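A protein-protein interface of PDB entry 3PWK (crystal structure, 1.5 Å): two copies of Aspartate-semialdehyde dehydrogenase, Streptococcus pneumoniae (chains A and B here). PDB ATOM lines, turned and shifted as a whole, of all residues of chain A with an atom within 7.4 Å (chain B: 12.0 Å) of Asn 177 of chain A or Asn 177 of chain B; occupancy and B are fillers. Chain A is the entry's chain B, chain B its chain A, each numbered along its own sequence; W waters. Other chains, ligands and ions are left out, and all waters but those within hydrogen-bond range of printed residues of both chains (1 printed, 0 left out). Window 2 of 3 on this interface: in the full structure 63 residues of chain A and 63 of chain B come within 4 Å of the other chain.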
ATOM      1  N   GLN A 169      16.146   1.882  -3.386  1.00  0.00           N
ATOM      2  CA  GLN A 169      16.687   2.194  -4.708  1.00  0.00           C
ATOM      3  C   GLN A 169      16.963   3.681  -4.871  1.00  0.00           C
ATOM      4  O   GLN A 169      18.016   4.048  -5.382  1.00  0.00           O
ATOM      5  CB  GLN A 169      15.745   1.697  -5.799  1.00  0.00           C
ATOM      6  CG  GLN A 169      15.603   0.180  -5.813  1.00  0.00           C
ATOM      7  CD  GLN A 169      14.567  -0.280  -6.817  1.00  0.00           C
ATOM      8  OE1 GLN A 169      13.457   0.268  -6.887  1.00  0.00           O
ATOM      9  NE2 GLN A 169      14.918  -1.288  -7.603  1.00  0.00           N
ATOM     10  N   GLU A 171      17.556   5.993  -2.492  1.00  0.00           N
ATOM     11  CA  GLU A 171      18.696   6.371  -1.649  1.00  0.00           C
ATOM     12  C   GLU A 171      20.026   5.948  -2.271  1.00  0.00           C
ATOM     13  O   GLU A 171      20.990   6.724  -2.281  1.00  0.00           O
ATOM     14  CB  GLU A 171      18.554   5.751  -0.256  1.00  0.00           C
ATOM     15  CG  GLU A 171      17.496   6.427   0.595  1.00  0.00           C
ATOM     16  CD  GLU A 171      17.277   5.756   1.941  1.00  0.00           C
ATOM     17  OE1 GLU A 171      18.094   4.894   2.325  1.00  0.00           O
ATOM     18  OE2 GLU A 171      16.271   6.080   2.611  1.00  0.00           O
ATOM     19  N   LEU A 172      20.088   4.714  -2.780  1.00  0.00           N
ATOM     20  CA  LEU A 172      21.337   4.222  -3.369  1.00  0.00           C
ATOM     21  C   LEU A 172      21.711   5.032  -4.603  1.00  0.00           C
ATOM     22  O   LEU A 172      22.894   5.323  -4.821  1.00  0.00           O
ATOM     23  CB  LEU A 172      21.245   2.740  -3.710  1.00  0.00           C
ATOM     24  CG  LEU A 172      21.235   1.796  -2.495  1.00  0.00           C
ATOM     25  CD1 LEU A 172      20.709   0.412  -2.875  1.00  0.00           C
ATOM     26  CD2 LEU A 172      22.630   1.695  -1.878  1.00  0.00           C
ATOM     27  N   ARG A 173      20.706   5.412  -5.394  1.00  0.00           N
ATOM     28  CA  ARG A 173      20.948   6.248  -6.567  1.00  0.00           C
ATOM     29  C   ARG A 173      21.446   7.624  -6.157  1.00  0.00           C
ATOM     30  O   ARG A 173      22.343   8.172  -6.806  1.00  0.00           O
ATOM     31  CB  ARG A 173      19.702   6.345  -7.451  1.00  0.00           C
ATOM     32  CG  ARG A 173      19.412   5.039  -8.186  1.00  0.00           C
ATOM     33  CD  ARG A 173      18.195   5.131  -9.090  1.00  0.00           C
ATOM     34  NE  ARG A 173      18.072   3.937  -9.930  1.00  0.00           N
ATOM     35  CZ  ARG A 173      17.044   3.090  -9.913  1.00  0.00           C
ATOM     36  NH1 ARG A 173      16.013   3.289  -9.100  1.00  0.00           N
ATOM     37  NH2 ARG A 173      17.046   2.043 -10.723  1.00  0.00           N
ATOM     38  N   GLU A 174      20.901   8.178  -5.076  1.00  0.00           N
ATOM     39  CA  GLU A 174      21.341   9.516  -4.642  1.00  0.00           C
ATOM     40  C   GLU A 174      22.805   9.486  -4.209  1.00  0.00           C
ATOM     41  O   GLU A 174      23.563  10.404  -4.500  1.00  0.00           O
ATOM     42  CB  GLU A 174      20.448  10.065  -3.530  1.00  0.00           C
ATOM     43  CG  GLU A 174      19.041  10.412  -4.012  1.00  0.00           C
ATOM     44  CD  GLU A 174      18.125  10.933  -2.923  1.00  0.00           C
ATOM     45  OE1 GLU A 174      18.594  11.213  -1.806  1.00  0.00           O
ATOM     46  OE2 GLU A 174      16.914  11.081  -3.195  1.00  0.00           O
ATOM     47  N   VAL A 175      23.210   8.419  -3.533  1.00  0.00           N
ATOM     48  CA  VAL A 175      24.613   8.281  -3.124  1.00  0.00           C
ATOM     49  C   VAL A 175      25.538   8.048  -4.318  1.00  0.00           C
ATOM     50  O   VAL A 175      26.515   8.774  -4.503  1.00  0.00           O
ATOM     51  CB  VAL A 175      24.784   7.121  -2.128  1.00  0.00           C
ATOM     52  CG1 VAL A 175      26.254   6.923  -1.787  1.00  0.00           C
ATOM     53  CG2 VAL A 175      23.976   7.384  -0.882  1.00  0.00           C
ATOM     54  N   LEU A 176      25.212   7.038  -5.127  1.00  0.00           N
ATOM     55  CA  LEU A 176      26.099   6.546  -6.176  1.00  0.00           C
ATOM     56  C   LEU A 176      26.160   7.401  -7.424  1.00  0.00           C
ATOM     57  O   LEU A 176      27.195   7.425  -8.093  1.00  0.00           O
ATOM     58  CB  LEU A 176      25.721   5.112  -6.560  1.00  0.00           C
ATOM     59  CG  LEU A 176      26.027   4.091  -5.464  1.00  0.00           C
ATOM     60  CD1 LEU A 176      25.135   2.888  -5.646  1.00  0.00           C
ATOM     61  CD2 LEU A 176      27.518   3.709  -5.470  1.00  0.00           C
ATOM     62  N   ASN A 177      25.052   8.077  -7.729  1.00  0.00           N
ATOM     63  CA  ASN A 177      24.928   8.887  -8.939  1.00  0.00           C
ATOM     64  C   ASN A 177      25.037  10.376  -8.659  1.00  0.00           C
ATOM     65  O   ASN A 177      25.514  11.137  -9.516  1.00  0.00           O
ATOM     66  CB  ASN A 177      23.601   8.597  -9.649  1.00  0.00           C
ATOM     67  CG  ASN A 177      23.512   7.179 -10.184  1.00  0.00           C
ATOM     68  OD1 ASN A 177      24.524   6.496 -10.363  1.00  0.00           O
ATOM     69  ND2 ASN A 177      22.290   6.733 -10.463  1.00  0.00           N
ATOM     70  N   ASP A 178      24.586  10.802  -7.478  1.00  0.00           N
ATOM     71  CA  ASP A 178      24.571  12.241  -7.149  1.00  0.00           C
ATOM     72  C   ASP A 178      25.646  12.635  -6.134  1.00  0.00           C
ATOM     73  O   ASP A 178      25.927  13.825  -5.943  1.00  0.00           O
ATOM     74  CB  ASP A 178      23.183  12.683  -6.655  1.00  0.00           C
ATOM     75  CG  ASP A 178      22.084  12.492  -7.703  1.00  0.00           C
ATOM     76  OD1 ASP A 178      22.384  12.565  -8.916  1.00  0.00           O
ATOM     77  OD2 ASP A 178      20.915  12.279  -7.308  1.00  0.00           O
ATOM     78  N   GLY A 179      26.247  11.642  -5.486  1.00  0.00           N
ATOM     79  CA  GLY A 179      27.303  11.889  -4.508  1.00  0.00           C
ATOM     80  C   GLY A 179      26.801  12.355  -3.152  1.00  0.00           C
ATOM     81  O   GLY A 179      27.531  13.015  -2.421  1.00  0.00           O
ATOM     82  N   VAL A 180      25.560  12.001  -2.811  1.00  0.00           N
ATOM     83  CA  VAL A 180      24.977  12.350  -1.520  1.00  0.00           C
ATOM     84  C   VAL A 180      25.636  11.475  -0.441  1.00  0.00           C
ATOM     85  O   VAL A 180      25.837  10.274  -0.659  1.00  0.00           O
ATOM     86  CB  VAL A 180      23.424  12.153  -1.552  1.00  0.00           C
ATOM     87  CG1 VAL A 180      22.774  12.408  -0.192  1.00  0.00           C
ATOM     88  CG2 VAL A 180      22.793  13.067  -2.612  1.00  0.00           C
ATOM     89  N   LEU B 166      35.722   0.071  -4.804  1.00  0.00           N
ATOM     90  CA  LEU B 166      35.420   0.370  -6.205  1.00  0.00           C
ATOM     91  C   LEU B 166      34.558  -0.721  -6.846  1.00  0.00           C
ATOM     92  O   LEU B 166      33.587  -0.411  -7.545  1.00  0.00           O
ATOM     93  CB  LEU B 166      36.709   0.583  -7.016  1.00  0.00           C
ATOM     94  CG  LEU B 166      37.593   1.757  -6.567  1.00  0.00           C
ATOM     95  CD1 LEU B 166      38.877   1.804  -7.414  1.00  0.00           C
ATOM     96  CD2 LEU B 166      36.842   3.090  -6.693  1.00  0.00           C
ATOM     97  N   GLU B 167      34.876  -1.985  -6.556  1.00  0.00           N
ATOM     98  CA  GLU B 167      34.106  -3.119  -7.074  1.00  0.00           C
ATOM     99  C   GLU B 167      32.653  -3.027  -6.619  1.00  0.00           C
ATOM    100  O   GLU B 167      31.726  -3.218  -7.416  1.00  0.00           O
ATOM    101  CB  GLU B 167      34.733  -4.437  -6.629  1.00  0.00           C
ATOM    102  CG  GLU B 167      33.897  -5.671  -6.941  1.00  0.00           C
ATOM    103  CD  GLU B 167      34.714  -6.950  -6.821  1.00  0.00           C
ATOM    104  OE1 GLU B 167      35.568  -7.184  -7.715  1.00  0.00           O
ATOM    105  OE2 GLU B 167      34.502  -7.713  -5.848  1.00  0.00           O
ATOM    106  N   THR B 168      32.457  -2.718  -5.340  1.00  0.00           N
ATOM    107  CA  THR B 168      31.108  -2.605  -4.778  1.00  0.00           C
ATOM    108  C   THR B 168      30.312  -1.484  -5.445  1.00  0.00           C
ATOM    109  O   THR B 168      29.158  -1.684  -5.828  1.00  0.00           O
ATOM    110  CB  THR B 168      31.180  -2.415  -3.245  1.00  0.00           C
ATOM    111  OG1 THR B 168      31.896  -3.521  -2.686  1.00  0.00           O
ATOM    112  CG2 THR B 168      29.789  -2.350  -2.617  1.00  0.00           C
ATOM    113  N   GLN B 169      30.936  -0.313  -5.589  1.00  0.00           N
ATOM    114  CA  GLN B 169      30.284   0.840  -6.211  1.00  0.00           C
ATOM    115  C   GLN B 169      29.920   0.568  -7.664  1.00  0.00           C
ATOM    116  O   GLN B 169      28.813   0.880  -8.111  1.00  0.00           O
ATOM    117  CB  GLN B 169      31.175   2.084  -6.088  1.00  0.00           C
ATOM    118  CG  GLN B 169      31.299   2.588  -4.640  1.00  0.00           C
ATOM    119  CD  GLN B 169      32.335   3.680  -4.489  1.00  0.00           C
ATOM    120  OE1 GLN B 169      33.449   3.561  -4.997  1.00  0.00           O
ATOM    121  NE2 GLN B 169      31.980   4.746  -3.780  1.00  0.00           N
ATOM    122  N   ARG B 170      30.855  -0.016  -8.396  1.00  0.00           N
ATOM    123  CA  ARG B 170      30.613  -0.366  -9.791  1.00  0.00           C
ATOM    124  C   ARG B 170      29.430  -1.345  -9.911  1.00  0.00           C
ATOM    125  O   ARG B 170      28.544  -1.172 -10.769  1.00  0.00           O
ATOM    126  CB  ARG B 170      31.899  -0.940 -10.407  1.00  0.00           C
ATOM    127  CG  ARG B 170      31.825  -1.271 -11.882  1.00  0.00           C
ATOM    128  CD  ARG B 170      31.527  -2.725 -12.140  1.00  0.00           C
ATOM    129  NE  ARG B 170      32.505  -3.646 -11.554  1.00  0.00           N
ATOM    130  CZ  ARG B 170      32.339  -4.965 -11.492  1.00  0.00           C
ATOM    131  NH1 ARG B 170      31.228  -5.521 -11.975  1.00  0.00           N
ATOM    132  NH2 ARG B 170      33.275  -5.727 -10.932  1.00  0.00           N
ATOM    133  N   GLU B 171      29.419  -2.364  -9.057  1.00  0.00           N
ATOM    134  CA  GLU B 171      28.390  -3.409  -9.141  1.00  0.00           C
ATOM    135  C   GLU B 171      27.022  -2.805  -8.881  1.00  0.00           C
ATOM    136  O   GLU B 171      26.056  -3.114  -9.578  1.00  0.00           O
ATOM    137  CB  GLU B 171      28.658  -4.546  -8.135  1.00  0.00           C
ATOM    138  CG  GLU B 171      29.773  -5.494  -8.545  1.00  0.00           C
ATOM    139  CD  GLU B 171      30.055  -6.549  -7.498  1.00  0.00           C
ATOM    140  OE1 GLU B 171      29.262  -6.696  -6.547  1.00  0.00           O
ATOM    141  OE2 GLU B 171      31.081  -7.234  -7.624  1.00  0.00           O
ATOM    142  N   LEU B 172      26.934  -1.967  -7.850  1.00  0.00           N
ATOM    143  CA  LEU B 172      25.662  -1.311  -7.516  1.00  0.00           C
ATOM    144  C   LEU B 172      25.153  -0.402  -8.631  1.00  0.00           C
ATOM    145  O   LEU B 172      23.957  -0.361  -8.907  1.00  0.00           O
ATOM    146  CB  LEU B 172      25.776  -0.535  -6.208  1.00  0.00           C
ATOM    147  CG  LEU B 172      25.890  -1.403  -4.945  1.00  0.00           C
ATOM    148  CD1 LEU B 172      26.382  -0.540  -3.819  1.00  0.00           C
ATOM    149  CD2 LEU B 172      24.544  -2.027  -4.629  1.00  0.00           C
ATOM    150  N   ARG B 173      26.069   0.323  -9.262  1.00  0.00           N
ATOM    151  CA  ARG B 173      25.731   1.144 -10.434  1.00  0.00           C
ATOM    152  C   ARG B 173      25.229   0.281 -11.591  1.00  0.00           C
ATOM    153  O   ARG B 173      24.260   0.643 -12.253  1.00  0.00           O
ATOM    154  CB  ARG B 173      26.923   2.015 -10.856  1.00  0.00           C
ATOM    155  CG  ARG B 173      27.195   3.174  -9.901  1.00  0.00           C
ATOM    156  CD  ARG B 173      28.398   4.029 -10.319  1.00  0.00           C
ATOM    157  NE  ARG B 173      28.625   5.094  -9.346  1.00  0.00           N
ATOM    158  CZ  ARG B 173      29.775   5.323  -8.706  1.00  0.00           C
ATOM    159  NH1 ARG B 173      30.849   4.568  -8.936  1.00  0.00           N
ATOM    160  NH2 ARG B 173      29.853   6.319  -7.826  1.00  0.00           N
ATOM    161  N   GLU B 174      25.859  -0.867 -11.824  1.00  0.00           N
ATOM    162  CA  GLU B 174      25.420  -1.751 -12.912  1.00  0.00           C
ATOM    163  C   GLU B 174      23.981  -2.232 -12.698  1.00  0.00           C
ATOM    164  O   GLU B 174      23.188  -2.298 -13.638  1.00  0.00           O
ATOM    165  CB  GLU B 174      26.381  -2.933 -13.100  1.00  0.00           C
ATOM    166  CG  GLU B 174      27.720  -2.516 -13.740  1.00  0.00           C
ATOM    167  CD  GLU B 174      28.661  -3.667 -14.086  1.00  0.00           C
ATOM    168  OE1 GLU B 174      29.283  -3.598 -15.157  1.00  0.00           O
ATOM    169  OE2 GLU B 174      28.833  -4.616 -13.307  1.00  0.00           O
ATOM    170  N   VAL B 175      23.645  -2.569 -11.458  1.00  0.00           N
ATOM    171  CA  VAL B 175      22.294  -3.021 -11.150  1.00  0.00           C
ATOM    172  C   VAL B 175      21.293  -1.874 -11.260  1.00  0.00           C
ATOM    173  O   VAL B 175      20.272  -1.986 -11.954  1.00  0.00           O
ATOM    174  CB  VAL B 175      22.228  -3.625  -9.742  1.00  0.00           C
ATOM    175  CG1 VAL B 175      20.779  -3.997  -9.390  1.00  0.00           C
ATOM    176  CG2 VAL B 175      23.142  -4.837  -9.657  1.00  0.00           C
ATOM    177  N   LEU B 176      21.603  -0.766 -10.591  1.00  0.00           N
ATOM    178  CA  LEU B 176      20.706   0.380 -10.537  1.00  0.00           C
ATOM    179  C   LEU B 176      20.595   1.154 -11.851  1.00  0.00           C
ATOM    180  O   LEU B 176      19.514   1.635 -12.189  1.00  0.00           O
ATOM    181  CB  LEU B 176      21.113   1.321  -9.401  1.00  0.00           C
ATOM    182  CG  LEU B 176      20.907   0.696  -8.015  1.00  0.00           C
ATOM    183  CD1 LEU B 176      21.723   1.444  -6.939  1.00  0.00           C
ATOM    184  CD2 LEU B 176      19.430   0.617  -7.646  1.00  0.00           C
ATOM    185  N   ASN B 177      21.694   1.242 -12.599  1.00  0.00           N
ATOM    186  CA  ASN B 177      21.720   2.078 -13.811  1.00  0.00           C
ATOM    187  C   ASN B 177      21.591   1.303 -15.116  1.00  0.00           C
ATOM    188  O   ASN B 177      21.095   1.837 -16.122  1.00  0.00           O
ATOM    189  CB  ASN B 177      22.983   2.958 -13.853  1.00  0.00           C
ATOM    190  CG  ASN B 177      23.112   3.866 -12.635  1.00  0.00           C
ATOM    191  OD1 ASN B 177      22.118   4.243 -12.009  1.00  0.00           O
ATOM    192  ND2 ASN B 177      24.350   4.219 -12.295  1.00  0.00           N
ATOM    193  N   ASP B 178      22.056   0.058 -15.114  1.00  0.00           N
ATOM    194  CA  ASP B 178      22.023  -0.769 -16.325  1.00  0.00           C
ATOM    195  C   ASP B 178      21.018  -1.919 -16.254  1.00  0.00           C
ATOM    196  O   ASP B 178      20.821  -2.634 -17.239  1.00  0.00           O
ATOM    197  CB  ASP B 178      23.424  -1.303 -16.635  1.00  0.00           C
ATOM    198  CG  ASP B 178      24.455  -0.196 -16.780  1.00  0.00           C
ATOM    199  OD1 ASP B 178      24.099   0.907 -17.245  1.00  0.00           O
ATOM    200  OD2 ASP B 178      25.629  -0.433 -16.429  1.00  0.00           O
ATOM    201  N   GLY B 179      20.388  -2.091 -15.095  1.00  0.00           N
ATOM    202  CA  GLY B 179      19.378  -3.129 -14.909  1.00  0.00           C
ATOM    203  C   GLY B 179      19.910  -4.551 -14.894  1.00  0.00           C
ATOM    204  O   GLY B 179      19.144  -5.498 -15.109  1.00  0.00           O
ATOM    205  N   VAL B 180      21.214  -4.703 -14.639  1.00  0.00           N
ATOM    206  CA  VAL B 180      21.848  -6.018 -14.498  1.00  0.00           C
ATOM    207  C   VAL B 180      21.286  -6.713 -13.241  1.00  0.00           C
ATOM    208  O   VAL B 180      21.146  -6.075 -12.190  1.00  0.00           O
ATOM    209  CB  VAL B 180      23.402  -5.873 -14.408  1.00  0.00           C
ATOM    210  CG1 VAL B 180      24.085  -7.220 -14.194  1.00  0.00           C
ATOM    211  CG2 VAL B 180      23.956  -5.194 -15.671  1.00  0.00           C
ATOM    212  N   LYS B 181      20.939  -7.999 -13.355  1.00  0.00           N
ATOM    213  CA  LYS B 181      20.514  -8.788 -12.197  1.00  0.00           C
ATOM    214  C   LYS B 181      21.739  -9.002 -11.316  1.00  0.00           C
ATOM    215  O   LYS B 181      22.813  -9.304 -11.834  1.00  0.00           O
ATOM    216  CB  LYS B 181      19.986 -10.160 -12.608  1.00  0.00           C
ATOM    217  CG  LYS B 181      18.664 -10.202 -13.344  1.00  0.00           C
ATOM    218  CD  LYS B 181      18.289 -11.683 -13.522  1.00  0.00           C
ATOM    219  CE  LYS B 181      17.284 -11.903 -14.621  1.00  0.00           C
ATOM    220  NZ  LYS B 181      17.240 -13.351 -14.977  1.00  0.00           N
ATOM    221  N   PRO B 182      21.592  -8.857  -9.987  1.00  0.00           N
ATOM    222  CA  PRO B 182      22.783  -9.052  -9.162  1.00  0.00           C
ATOM    223  C   PRO B 182      23.488 -10.394  -9.373  1.00  0.00           C
ATOM    224  O   PRO B 182      24.724 -10.423  -9.428  1.00  0.00           O
ATOM    225  CB  PRO B 182      22.245  -8.898  -7.744  1.00  0.00           C
ATOM    226  CG  PRO B 182      21.134  -7.910  -7.909  1.00  0.00           C
ATOM    227  CD  PRO B 182      20.479  -8.281  -9.206  1.00  0.00           C
ATOM    228  N   LEU B 185      26.184 -10.262 -12.145  1.00  0.00           N
ATOM    229  CA  LEU B 185      27.361  -9.393 -12.018  1.00  0.00           C
ATOM    230  C   LEU B 185      28.683 -10.156 -12.064  1.00  0.00           C
ATOM    231  O   LEU B 185      28.760 -11.322 -11.658  1.00  0.00           O
ATOM    232  CB  LEU B 185      27.288  -8.629 -10.695  1.00  0.00           C
ATOM    233  CG  LEU B 185      26.192  -7.574 -10.587  1.00  0.00           C
ATOM    234  CD1 LEU B 185      26.028  -7.152  -9.118  1.00  0.00           C
ATOM    235  CD2 LEU B 185      26.479  -6.367 -11.499  1.00  0.00           C
ATOM    236  N   ALA B 202      26.902  -6.701  -4.361  1.00  0.00           N
ATOM    237  CA  ALA B 202      25.738  -5.825  -4.496  1.00  0.00           C
ATOM    238  C   ALA B 202      24.437  -6.578  -4.179  1.00  0.00           C
ATOM    239  O   ALA B 202      24.189  -7.665  -4.722  1.00  0.00           O
ATOM    240  CB  ALA B 202      25.688  -5.228  -5.884  1.00  0.00           C
ATOM    241  N   PHE B 203      23.637  -6.018  -3.272  1.00  0.00           N
ATOM    242  CA  PHE B 203      22.362  -6.637  -2.853  1.00  0.00           C
ATOM    243  C   PHE B 203      22.541  -8.071  -2.346  1.00  0.00           C
ATOM    244  O   PHE B 203      21.636  -8.910  -2.462  1.00  0.00           O
ATOM    245  CB  PHE B 203      21.319  -6.551  -3.990  1.00  0.00           C
ATOM    246  CG  PHE B 203      21.056  -5.149  -4.431  1.00  0.00           C
ATOM    247  CD1 PHE B 203      20.276  -4.298  -3.658  1.00  0.00           C
ATOM    248  CD2 PHE B 203      21.654  -4.653  -5.585  1.00  0.00           C
ATOM    249  CE1 PHE B 203      20.046  -2.967  -4.054  1.00  0.00           C
ATOM    250  CE2 PHE B 203      21.433  -3.330  -5.983  1.00  0.00           C
ATOM    251  CZ  PHE B 203      20.614  -2.493  -5.218  1.00  0.00           C
ATOM    252  N   LEU B 249      30.111   0.447   2.703  1.00  0.00           N
ATOM    253  CA  LEU B 249      31.487   0.790   2.332  1.00  0.00           C
ATOM    254  C   LEU B 249      32.361   0.921   3.561  1.00  0.00           C
ATOM    255  O   LEU B 249      33.465   0.386   3.581  1.00  0.00           O
ATOM    256  CB  LEU B 249      31.566   2.058   1.490  1.00  0.00           C
ATOM    257  CG  LEU B 249      30.735   2.045   0.196  1.00  0.00           C
ATOM    258  CD1 LEU B 249      31.001   3.323  -0.610  1.00  0.00           C
ATOM    259  CD2 LEU B 249      31.032   0.810  -0.660  1.00  0.00           C
HETATM  260  O   HOH W   1      19.540   4.949 -12.251  1.00  0.00           O
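Of the printed residues of chain B, Leu 172 of chain A touches Leu 176 and Phe 203. Arg 173 of chain A touches just one residue of chain B: Leu 176 (2.9 Å). Val 175 of chain A touches none of the printed residues of chain B. Of chain B, only Leu 172, Arg 173 and Leu 176 come within 4 Å of Leu 176 of chain A. No residue of chain B comes within 4 Å of Asp 178 of chain A. Gly 179 of chain A touches none of the printed residues of chain B. Of the printed residues of chain A, Leu 172 of chain B touches Leu 176 (3.5 Å). Of the printed residues of chain A, Arg 173 of chain B touches Leu 176 (2.9 Å). Printed residues of chain A within 4 Å of Leu 176 of chain B: Leu 172, Arg 173 and Leu 176. Of the printed residues of chain A, Asn 177 of chain B touches Asn 177 (2.9 Å). Of the printed residues of chain A, Phe 203 of chain B touches Leu 172 (3.6 Å). The nearest residue of chain B that does not touch Asn 177 of chain A is Arg 173 of chain B (4.3 Å). The nearest residue of chain A that does not touch Asn 177 of chain B is Arg 173 of chain A (4.6 Å).
Among the printed residues, merely in contact across the chains: Leu 172 of chain A with Leu 176 of chain B (3.5 Å), Leu 172 of chain A with Phe 203 of chain B (3.6 Å), Leu 176 of chain A with Leu 172 of chain B (3.5 Å) and Leu 176 of chain A with Leu 176 of chain B (3.9 Å).
NH2 of Arg 173 of chain B sits at hydrogen-bond distance from O of Leu 176 of chain A (2.9 Å). ND2 of Asn 177 of chain A is in hydrogen-bond range of OD1 of Asn 177 of chain B, at 2.9 Å. The backbone carbonyl oxygen (O) of Leu 176 of chain B sits at hydrogen-bond distance from the guanidinium group (NH2) of Arg 173 of chain A.
Water W1 lies within hydrogen-bond range of OD1 of Asn 177 of chain B, NE of Arg 173 of chain A and O of Leu 176 of chain B.
Leu 172 of chain A touches Leu 176 of chain B, and with the chains exchanged Leu 176 of chain A touches Leu 172 of chain B. Arg 173 of chain A touches Leu 176 of chain B, and with the chains exchanged Leu 176 of chain A touches Arg 173 of chain B. Leu 176 of chain B touches its own counterpart, Leu 176 of chain A. Asn 177 of chain A touches its own counterpart, Asn 177 of chain B. Positions printed for both chains: 169, 171, 172, 173, 174, 175, 176, 177, 178, 179 and 180. Of the 7 pairs that touch across the chains among the printed residues, 6 have their exchanged pair printed and touching as well.
Printed residues of chain B that touch a printed residue of chain A: Leu 172, Arg 173, Leu 176, Asn 177 and Phe 203. Hydrophobic or aromatic side chains of chain B within 4 Å of the printed part of chain A: Leu 172, Leu 176 and Phe 203. Printed residues of chain A that touch a printed residue of chain B: Leu 172, Arg 173, Leu 176 and Asn 177. Hydrophobic or aromatic side chains of chain A that line the printed part of chain B: Leu 172 and Leu 176. Along chain A the printed residues that touch a printed residue of chain B span positions 172 to 177. Among the printed residues, no Asp or Glu carboxylate lies within 4 Å of a Lys or Arg side-chain nitrogen of the other chain.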
